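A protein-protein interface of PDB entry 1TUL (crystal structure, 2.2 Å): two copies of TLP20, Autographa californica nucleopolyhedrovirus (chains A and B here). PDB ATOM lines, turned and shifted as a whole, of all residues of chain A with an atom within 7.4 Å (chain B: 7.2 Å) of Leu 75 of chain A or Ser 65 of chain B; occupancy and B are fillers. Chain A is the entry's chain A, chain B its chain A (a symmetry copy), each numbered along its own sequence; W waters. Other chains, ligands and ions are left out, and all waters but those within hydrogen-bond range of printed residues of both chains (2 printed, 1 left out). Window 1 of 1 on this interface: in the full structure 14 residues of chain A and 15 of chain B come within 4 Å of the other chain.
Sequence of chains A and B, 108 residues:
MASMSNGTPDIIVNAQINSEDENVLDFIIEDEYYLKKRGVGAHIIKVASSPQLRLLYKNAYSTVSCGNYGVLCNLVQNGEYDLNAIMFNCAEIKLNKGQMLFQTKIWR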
ATOM      1  N   LEU A  53      -6.173 -27.011 -35.216  1.00  0.00           N
ATOM      2  CA  LEU A  53      -6.119 -26.297 -33.955  1.00  0.00           C
ATOM      3  C   LEU A  53      -7.231 -26.674 -33.017  1.00  0.00           C
ATOM      4  O   LEU A  53      -7.170 -26.469 -31.808  1.00  0.00           O
ATOM      5  CB  LEU A  53      -6.051 -24.743 -34.153  1.00  0.00           C
ATOM      6  CG  LEU A  53      -4.790 -24.255 -34.838  1.00  0.00           C
ATOM      7  CD1 LEU A  53      -4.813 -22.754 -34.983  1.00  0.00           C
ATOM      8  CD2 LEU A  53      -3.585 -24.623 -34.009  1.00  0.00           C
ATOM      9  N   ARG A  54      -8.269 -27.235 -33.583  1.00  0.00           N
ATOM     10  CA  ARG A  54      -9.421 -27.572 -32.799  1.00  0.00           C
ATOM     11  C   ARG A  54      -9.096 -28.465 -31.630  1.00  0.00           C
ATOM     12  O   ARG A  54      -9.785 -28.496 -30.610  1.00  0.00           O
ATOM     13  CB  ARG A  54     -10.432 -28.266 -33.688  1.00  0.00           C
ATOM     14  CG  ARG A  54     -11.862 -28.002 -33.272  1.00  0.00           C
ATOM     15  CD  ARG A  54     -12.852 -28.557 -34.297  1.00  0.00           C
ATOM     16  NE  ARG A  54     -13.312 -29.905 -33.977  1.00  0.00           N
ATOM     17  CZ  ARG A  54     -14.393 -30.135 -33.247  1.00  0.00           C
ATOM     18  NH1 ARG A  54     -15.126 -29.133 -32.756  1.00  0.00           N
ATOM     19  NH2 ARG A  54     -14.760 -31.392 -32.999  1.00  0.00           N
ATOM     20  N   LEU A  55      -8.062 -29.243 -31.823  1.00  0.00           N
ATOM     21  CA  LEU A  55      -7.621 -30.190 -30.806  1.00  0.00           C
ATOM     22  C   LEU A  55      -7.285 -29.543 -29.475  1.00  0.00           C
ATOM     23  O   LEU A  55      -7.396 -30.188 -28.439  1.00  0.00           O
ATOM     24  CB  LEU A  55      -6.360 -30.920 -31.288  1.00  0.00           C
ATOM     25  CG  LEU A  55      -6.597 -32.060 -32.260  1.00  0.00           C
ATOM     26  CD1 LEU A  55      -6.538 -31.555 -33.708  1.00  0.00           C
ATOM     27  CD2 LEU A  55      -5.501 -33.082 -32.034  1.00  0.00           C
ATOM     28  N   LEU A  56      -6.848 -28.286 -29.528  1.00  0.00           N
ATOM     29  CA  LEU A  56      -6.428 -27.507 -28.363  1.00  0.00           C
ATOM     30  C   LEU A  56      -7.598 -27.055 -27.516  1.00  0.00           C
ATOM     31  O   LEU A  56      -7.464 -26.626 -26.386  1.00  0.00           O
ATOM     32  CB  LEU A  56      -5.606 -26.307 -28.816  1.00  0.00           C
ATOM     33  CG  LEU A  56      -4.262 -26.747 -29.394  1.00  0.00           C
ATOM     34  CD1 LEU A  56      -3.454 -25.520 -29.768  1.00  0.00           C
ATOM     35  CD2 LEU A  56      -3.469 -27.528 -28.355  1.00  0.00           C
ATOM     36  N   TYR A  57      -8.760 -27.148 -28.103  1.00  0.00           N
ATOM     37  CA  TYR A  57      -9.942 -26.708 -27.432  1.00  0.00           C
ATOM     38  C   TYR A  57     -10.708 -27.865 -26.815  1.00  0.00           C
ATOM     39  O   TYR A  57     -11.718 -27.640 -26.174  1.00  0.00           O
ATOM     40  CB  TYR A  57     -10.843 -25.985 -28.443  1.00  0.00           C
ATOM     41  CG  TYR A  57     -10.246 -24.654 -28.840  1.00  0.00           C
ATOM     42  CD1 TYR A  57      -9.216 -24.578 -29.778  1.00  0.00           C
ATOM     43  CD2 TYR A  57     -10.723 -23.475 -28.268  1.00  0.00           C
ATOM     44  CE1 TYR A  57      -8.637 -23.360 -30.126  1.00  0.00           C
ATOM     45  CE2 TYR A  57     -10.180 -22.241 -28.612  1.00  0.00           C
ATOM     46  CZ  TYR A  57      -9.137 -22.206 -29.530  1.00  0.00           C
ATOM     47  OH  TYR A  57      -8.593 -21.035 -29.845  1.00  0.00           O
ATOM     48  N   LYS A  58     -10.199 -29.086 -26.982  1.00  0.00           N
ATOM     49  CA  LYS A  58     -10.821 -30.298 -26.471  1.00  0.00           C
ATOM     50  C   LYS A  58     -10.171 -30.894 -25.223  1.00  0.00           C
ATOM     51  O   LYS A  58     -10.782 -31.733 -24.566  1.00  0.00           O
ATOM     52  CB  LYS A  58     -10.737 -31.415 -27.501  1.00  0.00           C
ATOM     53  CG  LYS A  58     -11.694 -31.273 -28.658  1.00  0.00           C
ATOM     54  CD  LYS A  58     -12.578 -30.053 -28.536  1.00  0.00           C
ATOM     55  CE  LYS A  58     -13.780 -30.144 -29.452  1.00  0.00           C
ATOM     56  NZ  LYS A  58     -14.903 -29.310 -29.004  1.00  0.00           N
ATOM     57  N   ASN A  59      -8.905 -30.549 -24.940  1.00  0.00           N
ATOM     58  CA  ASN A  59      -8.181 -31.124 -23.811  1.00  0.00           C
ATOM     59  C   ASN A  59      -7.097 -30.217 -23.293  1.00  0.00           C
ATOM     60  O   ASN A  59      -6.642 -29.307 -23.973  1.00  0.00           O
ATOM     61  CB  ASN A  59      -7.407 -32.385 -24.277  1.00  0.00           C
ATOM     62  CG  ASN A  59      -8.254 -33.453 -24.957  1.00  0.00           C
ATOM     63  OD1 ASN A  59      -8.375 -33.517 -26.203  1.00  0.00           O
ATOM     64  ND2 ASN A  59      -8.828 -34.307 -24.127  1.00  0.00           N
ATOM     65  N   TYR A  61      -3.273 -29.113 -22.333  1.00  0.00           N
ATOM     66  CA  TYR A  61      -2.084 -29.217 -23.155  1.00  0.00           C
ATOM     67  C   TYR A  61      -0.914 -28.560 -22.509  1.00  0.00           C
ATOM     68  O   TYR A  61      -1.075 -27.792 -21.601  1.00  0.00           O
ATOM     69  CB  TYR A  61      -2.265 -28.633 -24.548  1.00  0.00           C
ATOM     70  CG  TYR A  61      -2.316 -27.115 -24.596  1.00  0.00           C
ATOM     71  CD1 TYR A  61      -3.528 -26.442 -24.424  1.00  0.00           C
ATOM     72  CD2 TYR A  61      -1.182 -26.353 -24.884  1.00  0.00           C
ATOM     73  CE1 TYR A  61      -3.615 -25.053 -24.489  1.00  0.00           C
ATOM     74  CE2 TYR A  61      -1.246 -24.960 -24.970  1.00  0.00           C
ATOM     75  CZ  TYR A  61      -2.471 -24.311 -24.789  1.00  0.00           C
ATOM     76  OH  TYR A  61      -2.541 -22.941 -24.865  1.00  0.00           O
ATOM     77  N   CYS A  73       1.045 -19.395 -24.889  1.00  0.00           N
ATOM     78  CA  CYS A  73      -0.133 -19.666 -25.756  1.00  0.00           C
ATOM     79  C   CYS A  73      -1.416 -19.451 -24.997  1.00  0.00           C
ATOM     80  O   CYS A  73      -1.521 -19.775 -23.824  1.00  0.00           O
ATOM     81  CB  CYS A  73      -0.228 -21.127 -26.203  1.00  0.00           C
ATOM     82  SG  CYS A  73       1.228 -21.605 -27.109  1.00  0.00           S
ATOM     83  N   ASN A  74      -2.414 -18.946 -25.687  1.00  0.00           N
ATOM     84  CA  ASN A  74      -3.696 -18.774 -25.043  1.00  0.00           C
ATOM     85  C   ASN A  74      -4.731 -19.235 -26.037  1.00  0.00           C
ATOM     86  O   ASN A  74      -4.568 -18.967 -27.225  1.00  0.00           O
ATOM     87  CB  ASN A  74      -4.005 -17.280 -24.834  1.00  0.00           C
ATOM     88  CG  ASN A  74      -3.605 -16.644 -23.513  1.00  0.00           C
ATOM     89  OD1 ASN A  74      -3.883 -15.468 -23.316  1.00  0.00           O
ATOM     90  ND2 ASN A  74      -2.956 -17.354 -22.609  1.00  0.00           N
ATOM     91  N   LEU A  75      -5.804 -19.866 -25.591  1.00  0.00           N
ATOM     92  CA  LEU A  75      -6.871 -20.213 -26.527  1.00  0.00           C
ATOM     93  C   LEU A  75      -7.585 -18.880 -26.816  1.00  0.00           C
ATOM     94  O   LEU A  75      -7.298 -17.896 -26.132  1.00  0.00           O
ATOM     95  CB  LEU A  75      -7.878 -21.229 -25.950  1.00  0.00           C
ATOM     96  CG  LEU A  75      -7.277 -22.580 -25.511  1.00  0.00           C
ATOM     97  CD1 LEU A  75      -8.375 -23.479 -24.947  1.00  0.00           C
ATOM     98  CD2 LEU A  75      -6.646 -23.302 -26.677  1.00  0.00           C
ATOM     99  N   VAL A  76      -8.476 -18.825 -27.835  1.00  0.00           N
ATOM    100  CA  VAL A  76      -9.224 -17.611 -28.155  1.00  0.00           C
ATOM    101  C   VAL A  76     -10.710 -17.828 -27.893  1.00  0.00           C
ATOM    102  O   VAL A  76     -11.247 -18.923 -28.076  1.00  0.00           O
ATOM    103  CB  VAL A  76      -8.929 -17.000 -29.518  1.00  0.00           C
ATOM    104  CG1 VAL A  76      -7.448 -17.155 -29.863  1.00  0.00           C
ATOM    105  CG2 VAL A  76      -9.734 -17.770 -30.540  1.00  0.00           C
ATOM    106  N   GLN A  77     -11.385 -16.816 -27.404  1.00  0.00           N
ATOM    107  CA  GLN A  77     -12.784 -16.982 -27.061  1.00  0.00           C
ATOM    108  C   GLN A  77     -13.633 -17.500 -28.225  1.00  0.00           C
ATOM    109  O   GLN A  77     -14.396 -18.469 -28.158  1.00  0.00           O
ATOM    110  CB  GLN A  77     -13.308 -15.631 -26.615  1.00  0.00           C
ATOM    111  CG  GLN A  77     -14.548 -15.705 -25.716  1.00  0.00           C
ATOM    112  CD  GLN A  77     -15.097 -14.311 -25.420  1.00  0.00           C
ATOM    113  OE1 GLN A  77     -15.845 -14.130 -24.452  1.00  0.00           O
ATOM    114  NE2 GLN A  77     -14.697 -13.311 -26.227  1.00  0.00           N
ATOM    115  N   ASN A  78     -13.479 -16.826 -29.324  1.00  0.00           N
ATOM    116  CA  ASN A  78     -14.224 -17.137 -30.517  1.00  0.00           C
ATOM    117  C   ASN A  78     -13.690 -18.263 -31.404  1.00  0.00           C
ATOM    118  O   ASN A  78     -12.699 -18.097 -32.111  1.00  0.00           O
ATOM    119  CB  ASN A  78     -14.309 -15.858 -31.352  1.00  0.00           C
ATOM    120  CG  ASN A  78     -15.694 -15.654 -31.894  1.00  0.00           C
ATOM    121  OD1 ASN A  78     -15.897 -14.991 -32.940  1.00  0.00           O
ATOM    122  ND2 ASN A  78     -16.658 -16.213 -31.144  1.00  0.00           N
ATOM    123  N   GLY A  79     -14.359 -19.389 -31.445  1.00  0.00           N
ATOM    124  CA  GLY A  79     -13.898 -20.405 -32.364  1.00  0.00           C
ATOM    125  C   GLY A  79     -12.660 -21.161 -31.932  1.00  0.00           C
ATOM    126  O   GLY A  79     -11.806 -20.655 -31.196  1.00  0.00           O
ATOM    127  N   ASP A  82      -8.149 -21.036 -33.859  1.00  0.00           N
ATOM    128  CA  ASP A  82      -7.152 -20.015 -33.718  1.00  0.00           C
ATOM    129  C   ASP A  82      -6.363 -20.178 -32.457  1.00  0.00           C
ATOM    130  O   ASP A  82      -6.747 -20.908 -31.558  1.00  0.00           O
ATOM    131  CB  ASP A  82      -7.785 -18.648 -33.696  1.00  0.00           C
ATOM    132  CG  ASP A  82      -8.211 -18.247 -35.060  1.00  0.00           C
ATOM    133  OD1 ASP A  82      -7.193 -17.957 -35.848  1.00  0.00           O
ATOM    134  OD2 ASP A  82      -9.383 -18.206 -35.377  1.00  0.00           O
ATOM    135  N   LEU A  83      -5.290 -19.452 -32.390  1.00  0.00           N
ATOM    136  CA  LEU A  83      -4.466 -19.503 -31.217  1.00  0.00           C
ATOM    137  C   LEU A  83      -3.669 -18.213 -31.107  1.00  0.00           C
ATOM    138  O   LEU A  83      -3.248 -17.673 -32.101  1.00  0.00           O
ATOM    139  CB  LEU A  83      -3.516 -20.698 -31.307  1.00  0.00           C
ATOM    140  CG  LEU A  83      -2.774 -21.026 -30.013  1.00  0.00           C
ATOM    141  CD1 LEU A  83      -3.753 -21.674 -29.046  1.00  0.00           C
ATOM    142  CD2 LEU A  83      -1.638 -22.019 -30.331  1.00  0.00           C
ATOM    143  N   ASN A  84      -3.489 -17.724 -29.878  1.00  0.00           N
ATOM    144  CA  ASN A  84      -2.673 -16.561 -29.589  1.00  0.00           C
ATOM    145  C   ASN A  84      -1.339 -17.058 -29.050  1.00  0.00           C
ATOM    146  O   ASN A  84      -1.304 -17.999 -28.273  1.00  0.00           O
ATOM    147  CB  ASN A  84      -3.263 -15.600 -28.511  1.00  0.00           C
ATOM    148  CG  ASN A  84      -4.313 -14.631 -29.010  1.00  0.00           C
ATOM    149  OD1 ASN A  84      -4.651 -14.621 -30.214  1.00  0.00           O
ATOM    150  ND2 ASN A  84      -4.854 -13.843 -28.085  1.00  0.00           N
ATOM    151  N   SER B  62      -7.063 -24.277 -18.964  1.00  0.00           N
ATOM    152  CA  SER B  62      -6.480 -23.569 -20.089  1.00  0.00           C
ATOM    153  C   SER B  62      -6.973 -22.136 -20.067  1.00  0.00           C
ATOM    154  O   SER B  62      -8.163 -21.903 -19.847  1.00  0.00           O
ATOM    155  CB  SER B  62      -6.871 -24.188 -21.403  1.00  0.00           C
ATOM    156  OG  SER B  62      -6.405 -25.519 -21.470  1.00  0.00           O
ATOM    157  N   THR B  63      -6.057 -21.198 -20.278  1.00  0.00           N
ATOM    158  CA  THR B  63      -6.392 -19.783 -20.325  1.00  0.00           C
ATOM    159  C   THR B  63      -6.867 -19.409 -21.726  1.00  0.00           C
ATOM    160  O   THR B  63      -6.240 -19.763 -22.712  1.00  0.00           O
ATOM    161  CB  THR B  63      -5.151 -18.961 -19.991  1.00  0.00           C
ATOM    162  OG1 THR B  63      -4.710 -19.330 -18.712  1.00  0.00           O
ATOM    163  CG2 THR B  63      -5.479 -17.492 -20.028  1.00  0.00           C
ATOM    164  N   VAL B  64      -7.992 -18.717 -21.800  1.00  0.00           N
ATOM    165  CA  VAL B  64      -8.581 -18.281 -23.051  1.00  0.00           C
ATOM    166  C   VAL B  64      -8.492 -16.782 -23.124  1.00  0.00           C
ATOM    167  O   VAL B  64      -8.978 -16.111 -22.220  1.00  0.00           O
ATOM    168  CB  VAL B  64     -10.077 -18.591 -23.078  1.00  0.00           C
ATOM    169  CG1 VAL B  64     -10.683 -18.206 -24.422  1.00  0.00           C
ATOM    170  CG2 VAL B  64     -10.335 -20.061 -22.843  1.00  0.00           C
ATOM    171  N   SER B  65      -7.930 -16.246 -24.195  1.00  0.00           N
ATOM    172  CA  SER B  65      -7.845 -14.778 -24.347  1.00  0.00           C
ATOM    173  C   SER B  65      -9.079 -14.201 -25.082  1.00  0.00           C
ATOM    174  O   SER B  65      -9.563 -14.810 -26.039  1.00  0.00           O
ATOM    175  CB  SER B  65      -6.566 -14.375 -25.058  1.00  0.00           C
ATOM    176  OG  SER B  65      -6.586 -12.993 -25.240  1.00  0.00           O
ATOM    177  N   CYS B  66      -9.623 -13.052 -24.634  1.00  0.00           N
ATOM    178  CA  CYS B  66     -10.818 -12.499 -25.293  1.00  0.00           C
ATOM    179  C   CYS B  66     -10.505 -11.425 -26.287  1.00  0.00           C
ATOM    180  O   CYS B  66     -11.376 -10.691 -26.701  1.00  0.00           O
ATOM    181  CB  CYS B  66     -11.921 -12.013 -24.339  1.00  0.00           C
ATOM    182  SG  CYS B  66     -12.410 -13.332 -23.202  1.00  0.00           S
ATOM    183  N   GLY B  67      -9.253 -11.347 -26.674  1.00  0.00           N
ATOM    184  CA  GLY B  67      -8.859 -10.354 -27.623  1.00  0.00           C
ATOM    185  C   GLY B  67      -7.441 -10.517 -28.127  1.00  0.00           C
ATOM    186  O   GLY B  67      -6.869 -11.606 -28.157  1.00  0.00           O
ATOM    187  N   ASN B  68      -6.893  -9.394 -28.533  1.00  0.00           N
ATOM    188  CA  ASN B  68      -5.581  -9.319 -29.107  1.00  0.00           C
ATOM    189  C   ASN B  68      -4.488  -9.101 -28.101  1.00  0.00           C
ATOM    190  O   ASN B  68      -3.788  -8.086 -28.121  1.00  0.00           O
ATOM    191  CB  ASN B  68      -5.569  -8.171 -30.101  1.00  0.00           C
ATOM    192  CG  ASN B  68      -4.435  -8.398 -31.033  1.00  0.00           C
ATOM    193  OD1 ASN B  68      -3.858  -7.438 -31.574  1.00  0.00           O
ATOM    194  ND2 ASN B  68      -4.071  -9.676 -31.155  1.00  0.00           N
ATOM    195  N   TYR B  69      -4.354 -10.067 -27.227  1.00  0.00           N
ATOM    196  CA  TYR B  69      -3.372 -10.005 -26.183  1.00  0.00           C
ATOM    197  C   TYR B  69      -3.221 -11.391 -25.593  1.00  0.00           C
ATOM    198  O   TYR B  69      -3.977 -12.310 -25.866  1.00  0.00           O
ATOM    199  CB  TYR B  69      -3.811  -8.985 -25.122  1.00  0.00           C
ATOM    200  CG  TYR B  69      -5.265  -9.177 -24.737  1.00  0.00           C
ATOM    201  CD1 TYR B  69      -5.663 -10.203 -23.876  1.00  0.00           C
ATOM    202  CD2 TYR B  69      -6.255  -8.329 -25.230  1.00  0.00           C
ATOM    203  CE1 TYR B  69      -7.000 -10.358 -23.516  1.00  0.00           C
ATOM    204  CE2 TYR B  69      -7.593  -8.444 -24.848  1.00  0.00           C
ATOM    205  CZ  TYR B  69      -7.969  -9.464 -23.973  1.00  0.00           C
ATOM    206  OH  TYR B  69      -9.292  -9.626 -23.602  1.00  0.00           O
ATOM    207  N   GLY B  70      -2.216 -11.561 -24.785  1.00  0.00           N
ATOM    208  CA  GLY B  70      -2.057 -12.858 -24.194  1.00  0.00           C
ATOM    209  C   GLY B  70      -2.121 -12.691 -22.710  1.00  0.00           C
ATOM    210  O   GLY B  70      -1.806 -11.639 -22.212  1.00  0.00           O
ATOM    211  N   VAL B  71      -2.564 -13.709 -21.996  1.00  0.00           N
ATOM    212  CA  VAL B  71      -2.644 -13.585 -20.560  1.00  0.00           C
ATOM    213  C   VAL B  71      -1.931 -14.751 -19.939  1.00  0.00           C
ATOM    214  O   VAL B  71      -2.139 -15.891 -20.357  1.00  0.00           O
ATOM    215  CB  VAL B  71      -4.106 -13.588 -20.114  1.00  0.00           C
ATOM    216  CG1 VAL B  71      -4.211 -13.627 -18.606  1.00  0.00           C
ATOM    217  CG2 VAL B  71      -4.812 -12.345 -20.622  1.00  0.00           C
ATOM    218  N   PHE B  88      -0.272  -9.351 -21.629  1.00  0.00           N
ATOM    219  CA  PHE B  88       0.688  -8.903 -22.658  1.00  0.00           C
ATOM    220  C   PHE B  88      -0.085  -8.426 -23.846  1.00  0.00           C
ATOM    221  O   PHE B  88      -0.609  -9.197 -24.638  1.00  0.00           O
ATOM    222  CB  PHE B  88       1.720  -9.937 -23.120  1.00  0.00           C
ATOM    223  CG  PHE B  88       2.472 -10.475 -21.932  1.00  0.00           C
ATOM    224  CD1 PHE B  88       2.007 -11.572 -21.211  1.00  0.00           C
ATOM    225  CD2 PHE B  88       3.633  -9.849 -21.493  1.00  0.00           C
ATOM    226  CE1 PHE B  88       2.698 -12.056 -20.103  1.00  0.00           C
ATOM    227  CE2 PHE B  88       4.348 -10.320 -20.394  1.00  0.00           C
ATOM    228  CZ  PHE B  88       3.868 -11.420 -19.692  1.00  0.00           C
ATOM    229  N   MET B 100     -15.330  -8.764 -20.905  1.00  0.00           N
ATOM    230  CA  MET B 100     -14.655  -9.994 -20.496  1.00  0.00           C
ATOM    231  C   MET B 100     -13.220  -9.946 -20.959  1.00  0.00           C
ATOM    232  O   MET B 100     -12.949  -9.760 -22.138  1.00  0.00           O
ATOM    233  CB  MET B 100     -15.313 -11.205 -21.121  1.00  0.00           C
ATOM    234  CG  MET B 100     -14.864 -12.498 -20.508  1.00  0.00           C
ATOM    235  SD  MET B 100     -15.985 -13.827 -21.013  1.00  0.00           S
ATOM    236  CE  MET B 100     -17.605 -13.168 -20.574  1.00  0.00           C
ATOM    237  N   LEU B 101     -12.291 -10.098 -20.041  1.00  0.00           N
ATOM    238  CA  LEU B 101     -10.883 -10.032 -20.376  1.00  0.00           C
ATOM    239  C   LEU B 101     -10.355 -11.374 -20.803  1.00  0.00           C
ATOM    240  O   LEU B 101      -9.640 -11.531 -21.797  1.00  0.00           O
ATOM    241  CB  LEU B 101     -10.061  -9.487 -19.166  1.00  0.00           C
ATOM    242  CG  LEU B 101      -8.618  -9.193 -19.515  1.00  0.00           C
ATOM    243  CD1 LEU B 101      -8.527  -8.074 -20.543  1.00  0.00           C
ATOM    244  CD2 LEU B 101      -7.828  -8.842 -18.270  1.00  0.00           C
ATOM    245  N   PHE B 102     -10.687 -12.341 -19.995  1.00  0.00           N
ATOM    246  CA  PHE B 102     -10.263 -13.664 -20.272  1.00  0.00           C
ATOM    247  C   PHE B 102     -11.100 -14.641 -19.500  1.00  0.00           C
ATOM    248  O   PHE B 102     -11.904 -14.223 -18.661  1.00  0.00           O
ATOM    249  CB  PHE B 102      -8.770 -13.826 -19.989  1.00  0.00           C
ATOM    250  CG  PHE B 102      -8.373 -13.854 -18.510  1.00  0.00           C
ATOM    251  CD1 PHE B 102      -8.063 -12.665 -17.842  1.00  0.00           C
ATOM    252  CD2 PHE B 102      -8.273 -15.050 -17.790  1.00  0.00           C
ATOM    253  CE1 PHE B 102      -7.695 -12.632 -16.492  1.00  0.00           C
ATOM    254  CE2 PHE B 102      -7.906 -15.048 -16.440  1.00  0.00           C
ATOM    255  CZ  PHE B 102      -7.609 -13.841 -15.797  1.00  0.00           C
ATOM    256  N   GLN B 103     -10.910 -15.932 -19.836  1.00  0.00           N
ATOM    257  CA  GLN B 103     -11.547 -17.082 -19.244  1.00  0.00           C
ATOM    258  C   GLN B 103     -10.550 -18.174 -18.987  1.00  0.00           C
ATOM    259  O   GLN B 103      -9.495 -18.274 -19.638  1.00  0.00           O
ATOM    260  CB  GLN B 103     -12.627 -17.718 -20.158  1.00  0.00           C
ATOM    261  CG  GLN B 103     -13.529 -16.685 -20.829  1.00  0.00           C
ATOM    262  CD  GLN B 103     -14.484 -17.292 -21.824  1.00  0.00           C
ATOM    263  OE1 GLN B 103     -14.074 -17.770 -22.879  1.00  0.00           O
ATOM    264  NE2 GLN B 103     -15.761 -17.277 -21.471  1.00  0.00           N
ATOM    265  N   LYS B 105     -10.718 -22.327 -18.712  1.00  0.00           N
ATOM    266  CA  LYS B 105     -11.481 -23.550 -18.940  1.00  0.00           C
ATOM    267  C   LYS B 105     -10.815 -24.676 -18.157  1.00  0.00           C
ATOM    268  O   LYS B 105      -9.624 -24.940 -18.303  1.00  0.00           O
ATOM    269  CB  LYS B 105     -11.558 -23.837 -20.429  1.00  0.00           C
ATOM    270  CG  LYS B 105     -11.859 -25.273 -20.702  1.00  0.00           C
ATOM    271  CD  LYS B 105     -13.255 -25.469 -21.241  1.00  0.00           C
ATOM    272  CE  LYS B 105     -14.215 -25.911 -20.162  1.00  0.00           C
ATOM    273  NZ  LYS B 105     -13.523 -26.533 -19.023  1.00  0.00           N
ATOM    274  N   TRP B 107     -10.362 -28.496 -16.970  1.00  0.00           N
ATOM    275  CA  TRP B 107     -10.486 -29.846 -17.484  1.00  0.00           C
ATOM    276  C   TRP B 107     -10.706 -30.805 -16.345  1.00  0.00           C
ATOM    277  O   TRP B 107      -9.773 -31.195 -15.650  1.00  0.00           O
ATOM    278  CB  TRP B 107      -9.278 -30.286 -18.336  1.00  0.00           C
ATOM    279  CG  TRP B 107      -8.966 -29.224 -19.359  1.00  0.00           C
ATOM    280  CD1 TRP B 107      -8.010 -28.264 -19.325  1.00  0.00           C
ATOM    281  CD2 TRP B 107      -9.693 -29.006 -20.532  1.00  0.00           C
ATOM    282  NE1 TRP B 107      -8.115 -27.437 -20.400  1.00  0.00           N
ATOM    283  CE2 TRP B 107      -9.144 -27.872 -21.165  1.00  0.00           C
ATOM    284  CE3 TRP B 107     -10.806 -29.642 -21.065  1.00  0.00           C
ATOM    285  CZ2 TRP B 107      -9.647 -27.402 -22.370  1.00  0.00           C
ATOM    286  CZ3 TRP B 107     -11.305 -29.180 -22.250  1.00  0.00           C
ATOM    287  CH2 TRP B 107     -10.718 -28.079 -22.906  1.00  0.00           C
HETATM  288  O   HOH W   1      -7.020 -26.649 -23.945  1.00  0.00           O
HETATM  289  O   HOH W   2      -4.208 -21.678 -22.844  1.00  0.00           O
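Among the printed residues, pairs that only touch across the chains: Tyr 57 of chain A with Trp 107 of chain B (3.4 Å), Lys 58 of chain A with Trp 107 of chain B (3.5 Å), Asn 59 of chain A with Trp 107 of chain B (3.7 Å), Asn 74 of chain A with Thr 63 of chain B (3.6 Å), Asn 74 of chain A with Ser 65 of chain B (3.4 Å), Asn 74 of chain A with Gly 70 of chain B (3.3 Å), Leu 75 of chain A with Ser 62 of chain B (3.9 Å), Leu 75 of chain A with Val 64 of chain B (3.4 Å), Val 76 of chain A with Val 64 of chain B (3.5 Å), Val 76 of chain A with Ser 65 of chain B (3.5 Å), Gln 77 of chain A with Val 64 of chain B (3.4 Å) and Gln 77 of chain A with Gln 103 of chain B (3.5 Å).
Printed residues of chain A that touch a printed residue of chain B: Tyr 57, Lys 58, Asn 59, Asn 74, Leu 75, Val 76, Gln 77 and Asn 84.
Hydrophobic or aromatic side chains of chain A that line the printed part of chain B: Leu 75.
Hydrophobic or aromatic side chains of chain B that line the printed part of chain A: Val 64, Val 71, Met 100 and Trp 107.
Among the printed residues, 21 pairs touch across the chains.
Among the printed residues, no Asp or Glu carboxylate lies within 4 Å of a Lys or Arg side-chain nitrogen of the other chain.
No position is printed for both chains.
Water W1 lies within hydrogen-bond range of the backbone carbonyl oxygen of Leu 56 of chain A (2.5 Å), the backbone carbonyl oxygen of Asn 59 of chain A (2.7 Å) and the side-chain hydroxyl of Ser 62 of chain B (2.8 Å).
Water W2 lies within hydrogen-bond range of O of Thr 63 of chain B, OH of Tyr 61 of chain A and O of Cys 73 of chain A.
The backbone NH (N) of Val 76 of chain A sits at hydrogen-bond distance from the side-chain hydroxyl (OH) of Tyr 57 of chain A (3.0 Å).
The backbone carbonyl oxygen (O) of Asp 82 of chain A lies within hydrogen-bond range of the side-chain hydroxyl (OH) of Tyr 57 of chain A (2.5 Å).
The backbone carbonyl oxygen of Lys 105 of chain B is in hydrogen-bond range of the backbone NH of Ser 62 of chain B (2.7 Å).
The side-chain hydroxyl (OG) of Ser 62 of chain B is in hydrogen-bond range of the indole nitrogen (NE1) of Trp 107 of chain B.
The backbone NH (N) of Val 64 of chain B sits at hydrogen-bond distance from the backbone carbonyl oxygen (O) of Gln 103 of chain B, 2.7 Å away.
The backbone NH (N) of Phe 102 of chain B lies close to the side-chain sulfur (SG) of Cys 66 of chain B (3.8 Å).
The side-chain amide oxygen (OD1) of Asn 74 of chain A is in hydrogen-bond range of the backbone NH (N) of Val 71 of chain B, at 2.6 Å.
The backbone carbonyl oxygen of Thr 63 of chain B is in hydrogen-bond range of the backbone NH of Leu 75 of chain A (2.9 Å).
The backbone carbonyl oxygen (O) of Leu 75 of chain A is in hydrogen-bond range of the backbone NH (N) of Ser 65 of chain B (2.6 Å).
The backbone carbonyl oxygen (O) of Ser 65 of chain B is in hydrogen-bond range of the backbone NH (N) of Gln 77 of chain A, at 3.0 Å.
The side-chain amide oxygen (OE1) of Gln 77 of chain A lies close to the side-chain sulfur (SG) of Cys 66 of chain B (3.7 Å).
The side-chain sulfur of Met 100 of chain B lies close to the side-chain amide oxygen of Gln 77 of chain A (3.5 Å).
The side-chain hydroxyl (OG) of Ser 65 of chain B is in hydrogen-bond range of the side-chain amide nitrogen (ND2) of Asn 84 of chain A (3.4 Å).
The side-chain amide nitrogen (ND2) of Asn 84 of chain A is in hydrogen-bond range of the backbone carbonyl oxygen (O) of Gly 67 of chain B, 3.0 Å away.
The backbone carbonyl oxygen (O) of Tyr 69 of chain B is in hydrogen-bond range of the side-chain amide nitrogen (ND2) of Asn 84 of chain A, 2.8 Å away.
Leu 75 of chain A touches just these residues of chain B: Ser 62 (3.9 Å), Thr 63 (2.9 Å), Val 64 (3.4 Å) and Ser 65 (2.6 Å).
Of the printed residues of chain B, Val 76 of chain A touches Val 64 (3.5 Å) and Ser 65 (3.5 Å).
Of the printed residues of chain A, Val 71 of chain B touches Asn 74.
Of the printed residues of chain B, Asn 59 of chain A touches Trp 107 (3.7 Å).
Printed residues of chain B within 4 Å of Lys 58 of chain A: Trp 107 (3.5 Å).
Of the printed residues of chain B, Asn 74 of chain A touches Thr 63, Ser 65, Gly 70 and Val 71.
Tyr 61 of chain A touches none of the printed residues of chain B.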
